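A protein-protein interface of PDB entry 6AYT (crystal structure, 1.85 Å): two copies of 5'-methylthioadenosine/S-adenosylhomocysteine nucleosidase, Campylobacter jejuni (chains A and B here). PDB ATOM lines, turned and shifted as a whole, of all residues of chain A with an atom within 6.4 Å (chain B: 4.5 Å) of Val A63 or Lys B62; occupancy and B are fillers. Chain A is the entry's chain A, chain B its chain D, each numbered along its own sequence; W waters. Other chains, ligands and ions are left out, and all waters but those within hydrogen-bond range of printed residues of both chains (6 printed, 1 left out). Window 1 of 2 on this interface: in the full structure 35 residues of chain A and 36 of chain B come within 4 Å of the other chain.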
ATOM      1  N   ILE A  60      -1.723  20.839  -3.618  1.00  0.00           N
ATOM      2  CA  ILE A  60      -2.558  19.913  -2.852  1.00  0.00           C
ATOM      3  C   ILE A  60      -3.882  19.613  -3.537  1.00  0.00           C
ATOM      4  O   ILE A  60      -4.473  20.495  -4.156  1.00  0.00           O
ATOM      5  CB  ILE A  60      -2.915  20.578  -1.477  1.00  0.00           C
ATOM      6  CG1 ILE A  60      -1.687  20.875  -0.632  1.00  0.00           C
ATOM      7  CG2 ILE A  60      -3.925  19.781  -0.684  1.00  0.00           C
ATOM      8  CD1 ILE A  60      -0.644  19.825  -0.660  1.00  0.00           C
ATOM      9  N   GLY A  61      -4.335  18.362  -3.415  1.00  0.00           N
ATOM     10  CA  GLY A  61      -5.706  18.006  -3.754  1.00  0.00           C
ATOM     11  C   GLY A  61      -5.889  17.267  -5.055  1.00  0.00           C
ATOM     12  O   GLY A  61      -4.954  17.077  -5.842  1.00  0.00           O
ATOM     13  N   LYS A  62      -7.135  16.875  -5.280  1.00  0.00           N
ATOM     14  CA  LYS A  62      -7.468  15.977  -6.378  1.00  0.00           C
ATOM     15  C   LYS A  62      -7.317  16.652  -7.734  1.00  0.00           C
ATOM     16  O   LYS A  62      -6.738  16.068  -8.638  1.00  0.00           O
ATOM     17  CB  LYS A  62      -8.863  15.407  -6.206  1.00  0.00           C
ATOM     18  CG  LYS A  62      -9.041  14.532  -4.971  1.00  0.00           C
ATOM     19  CD  LYS A  62     -10.320  13.702  -5.032  1.00  0.00           C
ATOM     20  CE  LYS A  62     -11.560  14.586  -5.079  1.00  0.00           C
ATOM     21  NZ  LYS A  62     -12.838  13.839  -5.024  1.00  0.00           N
ATOM     22  N   VAL A  63      -7.811  17.882  -7.874  1.00  0.00           N
ATOM     23  CA  VAL A  63      -7.738  18.580  -9.164  1.00  0.00           C
ATOM     24  C   VAL A  63      -6.285  18.854  -9.553  1.00  0.00           C
ATOM     25  O   VAL A  63      -5.884  18.554 -10.681  1.00  0.00           O
ATOM     26  CB  VAL A  63      -8.575  19.878  -9.162  1.00  0.00           C
ATOM     27  CG1 VAL A  63      -8.343  20.689 -10.437  1.00  0.00           C
ATOM     28  CG2 VAL A  63     -10.051  19.532  -9.015  1.00  0.00           C
ATOM     29  N   ASN A  64      -5.505  19.413  -8.628  1.00  0.00           N
ATOM     30  CA  ASN A  64      -4.094  19.735  -8.901  1.00  0.00           C
ATOM     31  C   ASN A  64      -3.287  18.495  -9.295  1.00  0.00           C
ATOM     32  O   ASN A  64      -2.545  18.521 -10.275  1.00  0.00           O
ATOM     33  CB  ASN A  64      -3.436  20.433  -7.704  1.00  0.00           C
ATOM     34  CG  ASN A  64      -3.941  21.854  -7.495  1.00  0.00           C
ATOM     35  OD1 ASN A  64      -4.317  22.555  -8.454  1.00  0.00           O
ATOM     36  ND2 ASN A  64      -3.977  22.279  -6.244  1.00  0.00           N
ATOM     37  N   SER A  65      -3.451  17.418  -8.541  1.00  0.00           N
ATOM     38  CA  SER A  65      -2.725  16.168  -8.807  1.00  0.00           C
ATOM     39  C   SER A  65      -3.152  15.493 -10.130  1.00  0.00           C
ATOM     40  O   SER A  65      -2.296  14.973 -10.864  1.00  0.00           O
ATOM     41  CB  SER A  65      -2.828  15.209  -7.627  1.00  0.00           C
ATOM     42  OG  SER A  65      -4.167  14.865  -7.305  1.00  0.00           O
ATOM     43  N   THR A  66      -4.451  15.552 -10.441  1.00  0.00           N
ATOM     44  CA  THR A  66      -4.990  15.054 -11.709  1.00  0.00           C
ATOM     45  C   THR A  66      -4.327  15.782 -12.882  1.00  0.00           C
ATOM     46  O   THR A  66      -3.859  15.156 -13.836  1.00  0.00           O
ATOM     47  CB  THR A  66      -6.534  15.231 -11.784  1.00  0.00           C
ATOM     48  OG1 THR A  66      -7.163  14.472 -10.751  1.00  0.00           O
ATOM     49  CG2 THR A  66      -7.111  14.787 -13.117  1.00  0.00           C
ATOM     50  N   LEU A  67      -4.268  17.109 -12.788  1.00  0.00           N
ATOM     51  CA  LEU A  67      -3.676  17.924 -13.841  1.00  0.00           C
ATOM     52  C   LEU A  67      -2.199  17.602 -14.041  1.00  0.00           C
ATOM     53  O   LEU A  67      -1.765  17.421 -15.183  1.00  0.00           O
ATOM     54  CB  LEU A  67      -3.864  19.417 -13.546  1.00  0.00           C
ATOM     55  CG  LEU A  67      -3.258  20.410 -14.544  1.00  0.00           C
ATOM     56  CD1 LEU A  67      -3.818  20.170 -15.938  1.00  0.00           C
ATOM     57  CD2 LEU A  67      -3.469  21.827 -14.065  1.00  0.00           C
ATOM     58  N   SER A  68      -1.433  17.516 -12.944  1.00  0.00           N
ATOM     59  CA  SER A  68      -0.004  17.186 -13.027  1.00  0.00           C
ATOM     60  C   SER A  68       0.260  15.816 -13.637  1.00  0.00           C
ATOM     61  O   SER A  68       1.130  15.693 -14.500  1.00  0.00           O
ATOM     62  CB  SER A  68       0.692  17.293 -11.666  1.00  0.00           C
ATOM     63  OG  SER A  68       0.945  18.645 -11.343  1.00  0.00           O
ATOM     64  N   GLN A 107     -12.122   7.463  -3.894  1.00  0.00           N
ATOM     65  CA  GLN A 107     -12.429   8.838  -3.513  1.00  0.00           C
ATOM     66  C   GLN A 107     -13.600   8.806  -2.537  1.00  0.00           C
ATOM     67  O   GLN A 107     -14.769   8.618  -2.945  1.00  0.00           O
ATOM     68  CB  GLN A 107     -12.795   9.694  -4.728  1.00  0.00           C
ATOM     69  CG  GLN A 107     -11.660   9.886  -5.714  1.00  0.00           C
ATOM     70  CD  GLN A 107     -12.114  10.601  -6.979  1.00  0.00           C
ATOM     71  OE1 GLN A 107     -12.567  11.747  -6.925  1.00  0.00           O
ATOM     72  NE2 GLN A 107     -11.992   9.920  -8.129  1.00  0.00           N
ATOM     73  N   ASP A 109     -14.995  11.188  -0.917  1.00  0.00           N
ATOM     74  CA  ASP A 109     -15.825  12.391  -0.960  1.00  0.00           C
ATOM     75  C   ASP A 109     -16.558  12.601  -2.298  1.00  0.00           C
ATOM     76  O   ASP A 109     -17.076  13.694  -2.560  1.00  0.00           O
ATOM     77  CB  ASP A 109     -14.971  13.628  -0.585  1.00  0.00           C
ATOM     78  CG  ASP A 109     -13.889  13.956  -1.616  1.00  0.00           C
ATOM     79  OD1 ASP A 109     -13.583  13.120  -2.479  1.00  0.00           O
ATOM     80  OD2 ASP A 109     -13.322  15.068  -1.524  1.00  0.00           O
ATOM     81  N   LEU A 110     -16.576  11.571  -3.148  1.00  0.00           N
ATOM     82  CA  LEU A 110     -17.274  11.613  -4.425  1.00  0.00           C
ATOM     83  C   LEU A 110     -18.624  10.968  -4.201  1.00  0.00           C
ATOM     84  O   LEU A 110     -18.702   9.760  -3.986  1.00  0.00           O
ATOM     85  CB  LEU A 110     -16.455  10.911  -5.519  1.00  0.00           C
ATOM     86  CG  LEU A 110     -17.005  10.869  -6.940  1.00  0.00           C
ATOM     87  CD1 LEU A 110     -17.330  12.248  -7.483  1.00  0.00           C
ATOM     88  CD2 LEU A 110     -16.013  10.163  -7.854  1.00  0.00           C
ATOM     89  N   ASP A 159     -10.659  15.559  -0.738  1.00  0.00           N
ATOM     90  CA  ASP A 159     -10.128  16.929  -0.690  1.00  0.00           C
ATOM     91  C   ASP A 159     -10.262  17.600   0.691  1.00  0.00           C
ATOM     92  O   ASP A 159     -10.281  18.834   0.794  1.00  0.00           O
ATOM     93  CB  ASP A 159     -10.760  17.764  -1.819  1.00  0.00           C
ATOM     94  CG  ASP A 159      -9.957  17.713  -3.112  1.00  0.00           C
ATOM     95  OD1 ASP A 159      -8.770  17.309  -3.093  1.00  0.00           O
ATOM     96  OD2 ASP A 159     -10.515  18.099  -4.154  1.00  0.00           O
ATOM     97  N   MET A 182      -4.875  13.184  -0.196  1.00  0.00           N
ATOM     98  CA  MET A 182      -5.674  14.068  -1.036  1.00  0.00           C
ATOM     99  C   MET A 182      -5.319  14.014  -2.524  1.00  0.00           C
ATOM    100  O   MET A 182      -5.787  14.850  -3.288  1.00  0.00           O
ATOM    101  CB  MET A 182      -5.550  15.510  -0.484  1.00  0.00           C
ATOM    102  CG  MET A 182      -5.947  15.651   0.988  1.00  0.00           C
ATOM    103  SD  MET A 182      -5.702  17.315   1.681  1.00  0.00           S
ATOM    104  CE  MET A 182      -6.810  18.295   0.712  1.00  0.00           C
ATOM    105  N   SER A 186      -6.871  10.071  -7.508  1.00  0.00           N
ATOM    106  CA  SER A 186      -6.913  10.909  -8.691  1.00  0.00           C
ATOM    107  C   SER A 186      -5.719  10.644  -9.614  1.00  0.00           C
ATOM    108  O   SER A 186      -5.893  10.522 -10.824  1.00  0.00           O
ATOM    109  CB  SER A 186      -7.002  12.391  -8.287  1.00  0.00           C
ATOM    110  OG  SER A 186      -6.159  12.682  -7.197  1.00  0.00           O
ATOM    111  N   GLY B  61     -17.875  14.758 -12.002  1.00  0.00           N
ATOM    112  CA  GLY B  61     -16.998  15.128 -10.901  1.00  0.00           C
ATOM    113  C   GLY B  61     -15.724  15.837 -11.299  1.00  0.00           C
ATOM    114  O   GLY B  61     -15.399  15.988 -12.494  1.00  0.00           O
ATOM    115  N   LYS B  62     -14.983  16.242 -10.275  1.00  0.00           N
ATOM    116  CA  LYS B  62     -13.834  17.104 -10.462  1.00  0.00           C
ATOM    117  C   LYS B  62     -12.677  16.400 -11.171  1.00  0.00           C
ATOM    118  O   LYS B  62     -12.097  16.955 -12.092  1.00  0.00           O
ATOM    119  CB  LYS B  62     -13.375  17.693  -9.133  1.00  0.00           C
ATOM    120  CG  LYS B  62     -14.411  18.607  -8.470  1.00  0.00           C
ATOM    121  CD  LYS B  62     -13.814  19.446  -7.351  1.00  0.00           C
ATOM    122  CE  LYS B  62     -13.252  18.585  -6.226  1.00  0.00           C
ATOM    123  NZ  LYS B  62     -12.752  19.354  -5.059  1.00  0.00           N
ATOM    124  N   VAL B  63     -12.364  15.177 -10.768  1.00  0.00           N
ATOM    125  CA  VAL B  63     -11.238  14.446 -11.357  1.00  0.00           C
ATOM    126  C   VAL B  63     -11.495  14.146 -12.837  1.00  0.00           C
ATOM    127  O   VAL B  63     -10.635  14.420 -13.696  1.00  0.00           O
ATOM    128  CB  VAL B  63     -10.902  13.162 -10.577  1.00  0.00           C
ATOM    129  CG1 VAL B  63      -9.832  12.348 -11.294  1.00  0.00           C
ATOM    130  CG2 VAL B  63     -10.442  13.504  -9.168  1.00  0.00           C
ATOM    131  N   ASN B  64     -12.675  13.599 -13.140  1.00  0.00           N
ATOM    132  CA  ASN B  64     -13.029  13.251 -14.519  1.00  0.00           C
ATOM    133  C   ASN B  64     -12.996  14.472 -15.444  1.00  0.00           C
ATOM    134  O   ASN B  64     -12.414  14.412 -16.546  1.00  0.00           O
ATOM    135  CB  ASN B  64     -14.411  12.576 -14.594  1.00  0.00           C
ATOM    136  CG  ASN B  64     -14.417  11.171 -14.009  1.00  0.00           C
ATOM    137  OD1 ASN B  64     -13.418  10.449 -14.064  1.00  0.00           O
ATOM    138  ND2 ASN B  64     -15.543  10.781 -13.437  1.00  0.00           N
ATOM    139  N   SER B  65     -13.602  15.571 -14.993  1.00  0.00           N
ATOM    140  CA  SER B  65     -13.650  16.801 -15.788  1.00  0.00           C
ATOM    141  C   SER B  65     -12.269  17.447 -15.989  1.00  0.00           C
ATOM    142  O   SER B  65     -11.971  17.946 -17.086  1.00  0.00           O
ATOM    143  CB  SER B  65     -14.666  17.794 -15.209  1.00  0.00           C
ATOM    144  OG  SER B  65     -14.384  18.164 -13.870  1.00  0.00           O
ATOM    145  N   THR B  66     -11.431  17.404 -14.944  1.00  0.00           N
ATOM    146  CA  THR B  66     -10.049  17.890 -15.007  1.00  0.00           C
ATOM    147  C   THR B  66      -9.282  17.138 -16.102  1.00  0.00           C
ATOM    148  O   THR B  66      -8.617  17.752 -16.947  1.00  0.00           O
ATOM    149  CB  THR B  66      -9.329  17.731 -13.645  1.00  0.00           C
ATOM    150  OG1 THR B  66      -9.989  18.517 -12.644  1.00  0.00           O
ATOM    151  CG2 THR B  66      -7.857  18.147 -13.705  1.00  0.00           C
ATOM    152  N   GLN B 107     -13.979  25.740  -5.383  1.00  0.00           N
ATOM    153  CA  GLN B 107     -14.213  24.385  -4.898  1.00  0.00           C
ATOM    154  C   GLN B 107     -14.591  24.462  -3.420  1.00  0.00           C
ATOM    155  O   GLN B 107     -13.722  24.641  -2.563  1.00  0.00           O
ATOM    156  CB  GLN B 107     -12.977  23.507  -5.074  1.00  0.00           C
ATOM    157  CG  GLN B 107     -12.569  23.271  -6.518  1.00  0.00           C
ATOM    158  CD  GLN B 107     -11.253  22.530  -6.629  1.00  0.00           C
ATOM    159  OE1 GLN B 107     -11.134  21.403  -6.173  1.00  0.00           O
ATOM    160  NE2 GLN B 107     -10.258  23.157  -7.252  1.00  0.00           N
ATOM    161  N   ASP B 109     -15.493  22.141  -1.409  1.00  0.00           N
ATOM    162  CA  ASP B 109     -15.111  20.950  -0.660  1.00  0.00           C
ATOM    163  C   ASP B 109     -13.591  20.715  -0.579  1.00  0.00           C
ATOM    164  O   ASP B 109     -13.153  19.637  -0.197  1.00  0.00           O
ATOM    165  CB  ASP B 109     -15.839  19.712  -1.241  1.00  0.00           C
ATOM    166  CG  ASP B 109     -15.393  19.348  -2.655  1.00  0.00           C
ATOM    167  OD1 ASP B 109     -14.732  20.157  -3.328  1.00  0.00           O
ATOM    168  OD2 ASP B 109     -15.726  18.233  -3.111  1.00  0.00           O
ATOM    169  N   THR B 157     -18.283  24.630  -6.903  1.00  0.00           N
ATOM    170  CA  THR B 157     -18.082  23.284  -7.417  1.00  0.00           C
ATOM    171  C   THR B 157     -17.608  22.363  -6.297  1.00  0.00           C
ATOM    172  O   THR B 157     -16.795  22.746  -5.467  1.00  0.00           O
ATOM    173  CB  THR B 157     -17.026  23.301  -8.544  1.00  0.00           C
ATOM    174  OG1 THR B 157     -17.507  24.081  -9.638  1.00  0.00           O
ATOM    175  CG2 THR B 157     -16.692  21.894  -9.043  1.00  0.00           C
ATOM    176  N   GLY B 158     -18.111  21.131  -6.288  1.00  0.00           N
ATOM    177  CA  GLY B 158     -17.588  20.121  -5.380  1.00  0.00           C
ATOM    178  C   GLY B 158     -18.058  18.764  -5.834  1.00  0.00           C
ATOM    179  O   GLY B 158     -18.887  18.667  -6.729  1.00  0.00           O
ATOM    180  N   ASP B 159     -17.570  17.717  -5.185  1.00  0.00           N
ATOM    181  CA  ASP B 159     -17.862  16.348  -5.610  1.00  0.00           C
ATOM    182  C   ASP B 159     -19.071  15.711  -4.892  1.00  0.00           C
ATOM    183  O   ASP B 159     -19.179  14.482  -4.813  1.00  0.00           O
ATOM    184  CB  ASP B 159     -16.585  15.494  -5.501  1.00  0.00           C
ATOM    185  CG  ASP B 159     -15.762  15.496  -6.780  1.00  0.00           C
ATOM    186  OD1 ASP B 159     -16.276  15.885  -7.853  1.00  0.00           O
ATOM    187  OD2 ASP B 159     -14.583  15.087  -6.708  1.00  0.00           O
ATOM    188  N   MET B 182     -20.519  20.014 -10.229  1.00  0.00           N
ATOM    189  CA  MET B 182     -19.426  19.124  -9.845  1.00  0.00           C
ATOM    190  C   MET B 182     -18.225  19.140 -10.796  1.00  0.00           C
ATOM    191  O   MET B 182     -17.338  18.286 -10.685  1.00  0.00           O
ATOM    192  CB  MET B 182     -19.992  17.702  -9.692  1.00  0.00           C
ATOM    193  CG  MET B 182     -21.154  17.598  -8.686  1.00  0.00           C
ATOM    194  SD  MET B 182     -21.906  15.961  -8.579  1.00  0.00           S
ATOM    195  CE  MET B 182     -20.542  14.965  -8.004  1.00  0.00           C
ATOM    196  N   SER B 186     -13.007  22.981 -11.580  1.00  0.00           N
ATOM    197  CA  SER B 186     -11.927  22.114 -12.029  1.00  0.00           C
ATOM    198  C   SER B 186     -11.593  22.353 -13.509  1.00  0.00           C
ATOM    199  O   SER B 186     -10.427  22.448 -13.872  1.00  0.00           O
ATOM    200  CB  SER B 186     -12.264  20.643 -11.760  1.00  0.00           C
ATOM    201  OG  SER B 186     -13.614  20.366 -12.055  1.00  0.00           O
ATOM    202  N   LEU B 189     -10.028  25.896 -13.893  1.00  0.00           N
ATOM    203  CA  LEU B 189      -8.654  25.831 -13.402  1.00  0.00           C
ATOM    204  C   LEU B 189      -7.697  25.269 -14.455  1.00  0.00           C
ATOM    205  O   LEU B 189      -6.643  25.847 -14.693  1.00  0.00           O
ATOM    206  CB  LEU B 189      -8.584  25.004 -12.111  1.00  0.00           C
ATOM    207  CG  LEU B 189      -7.238  24.847 -11.384  1.00  0.00           C
ATOM    208  CD1 LEU B 189      -7.462  24.518  -9.912  1.00  0.00           C
ATOM    209  CD2 LEU B 189      -6.350  23.784 -12.025  1.00  0.00           C
HETATM  210  O   HOH W   1     -17.260  16.473  -1.721  1.00  0.00           O
HETATM  211  O   HOH W   2     -13.304  10.407 -10.671  1.00  0.00           O
HETATM  212  O   HOH W   3      -9.170  19.582  -5.788  1.00  0.00           O
HETATM  213  O   HOH W   4     -13.812  16.959   0.519  1.00  0.00           O
HETATM  214  O   HOH W   5      -7.371  22.666  -7.157  1.00  0.00           O
HETATM  215  O   HOH W   6     -13.697  13.505  -8.602  1.00  0.00           O
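Lys B62 touches Val A63 (CB to CG2, 3.8 Å). CG1 of Val A63 touches CD1 of Leu B189, at 3.96 Å. CD1 of Leu B189 touches OD1 of Asn A64 (3.98 Å). CG2 of Thr A66 touches CG2 of Thr B66 (3.5 Å). Leu A67 touches Thr B66. Val B63 touches Gln A107. OE1 of Gln A107 touches OD2 of Asp B159, at 3.9 Å. Asp B159 touches Leu A110. Asp A159 touches Gln B107. CG2 of Val B63 touches CB of Ser A186, 3.7 Å away.
Val A63 touches five residues of chain B. Of the printed residues of chain B, Asp A159 touches Lys B62, Gln B107 and Asp B109. Of the printed residues of chain A, Thr B66 touches Val A63, Thr A66 and Leu A67. Printed residues of chain B within 4 Å of Leu A67: Thr B66 (3.8 Å). Printed residues of chain B within 4 Å of Asn A64: Leu B189. Of the printed residues of chain B, Gln A107 touches Val B63 and Asp B159. Gly B158 touches none of the printed residues of chain A. Ile A60 touches none of the printed residues of chain B. The nearest printed residue of chain B that does not touch Val A63 is Val B63 (5.2 Å). The nearest residue of chain A that does not touch Lys B62 is Lys A62 (4.5 Å).
Printed residues of chain A that touch a printed residue of chain B: Lys A62, Val A63, Asn A64, Thr A66, Leu A67, Gln A107, Asp A109, Leu A110, Asp A159 and Ser A186. Hydrophobic or aromatic side chains of chain B that line the printed part of chain A: Val B63 and Leu B189. Among the printed residues, 19 pairs touch across the chains. Among the printed residues, Asp or Glu carboxylates within 4 Å of a Lys or Arg side-chain nitrogen of the other chain: Lys A62 with Asp B159 (2.7 Å) and Asp A159 with Lys B62 (2.7 Å).
Lys A62 touches Val B63, and with the chains exchanged Val A63 touches Lys B62. Val A63 touches Ser B186, and with the chains exchanged Ser A186 touches Val B63. Gln A107 touches Asp B159, and with the chains exchanged Asp A159 touches Gln B107. Asp A109 touches Asp B159, and with the chains exchanged Asp A159 touches Asp B109.
Water W3 lies within hydrogen-bond range of the side-chain carboxylate of Asp A159 (2.6 Å), the side-chain amide oxygen of Gln B107 (2.7 Å), the backbone NH of Val A63 (3.0 Å) and the backbone NH of Lys A62 (3.4 Å). Water W6 lies within hydrogen-bond range of the side-chain carboxylate of Asp B159, the side-chain amide oxygen of Gln A107, the backbone NH of Val B63 and the backbone NH of Lys B62. Water W1 lies within hydrogen-bond range of OD2 of Asp B109 (2.7 Å) and O of Asp A109 (2.9 Å). Water W4 lies within hydrogen-bond range of the side-chain carboxylate of Asp A109 (2.8 Å) and the backbone carbonyl oxygen of Asp B109 (2.8 Å). Water W2 lies within hydrogen-bond range of NE2 of Gln A107 (2.9 Å) and OD1 of Asn B64 (3.4 Å). Water W5 lies within hydrogen-bond range of NE2 of Gln B107 (2.9 Å) and OD1 of Asn A64 (3.3 Å).
The side-chain carboxylate (OD1) of Asp A159 is in hydrogen-bond range of the backbone NH (N) of Lys A62. The backbone NH (N) of Lys A62 is in hydrogen-bond range of the backbone carbonyl oxygen (O) of Met A182, at 3.1 Å. The side-chain hydroxyl (OG) of Ser A65 is in hydrogen-bond range of the side-chain hydroxyl (OG) of Ser A186 (3.0 Å). NZ of Lys B62 is in hydrogen-bond range of OE1 of Gln B107 (2.8 Å). OG of Ser B65 is in hydrogen-bond range of OG of Ser B186, 3.0 Å away. N of Asp B159 sits at hydrogen-bond distance from OD2 of Asp B109 (2.8 Å).
The side-chain carboxylate (OD2) of Asp B159 is in salt-bridge range of the side-chain amino group (NZ) of Lys A62 (2.7 Å). The side-chain amino group (NZ) of Lys B62 is in salt-bridge range of the side-chain carboxylate (OD2) of Asp A159, at 2.7 Å. The backbone carbonyl oxygen (O) of Asp A109 sits close to the backbone carbonyl oxygen (O) of Asp B159, 3.2 Å away. The backbone carbonyl oxygen of Asp A159 lies close to the backbone carbonyl oxygen of Asp B109.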
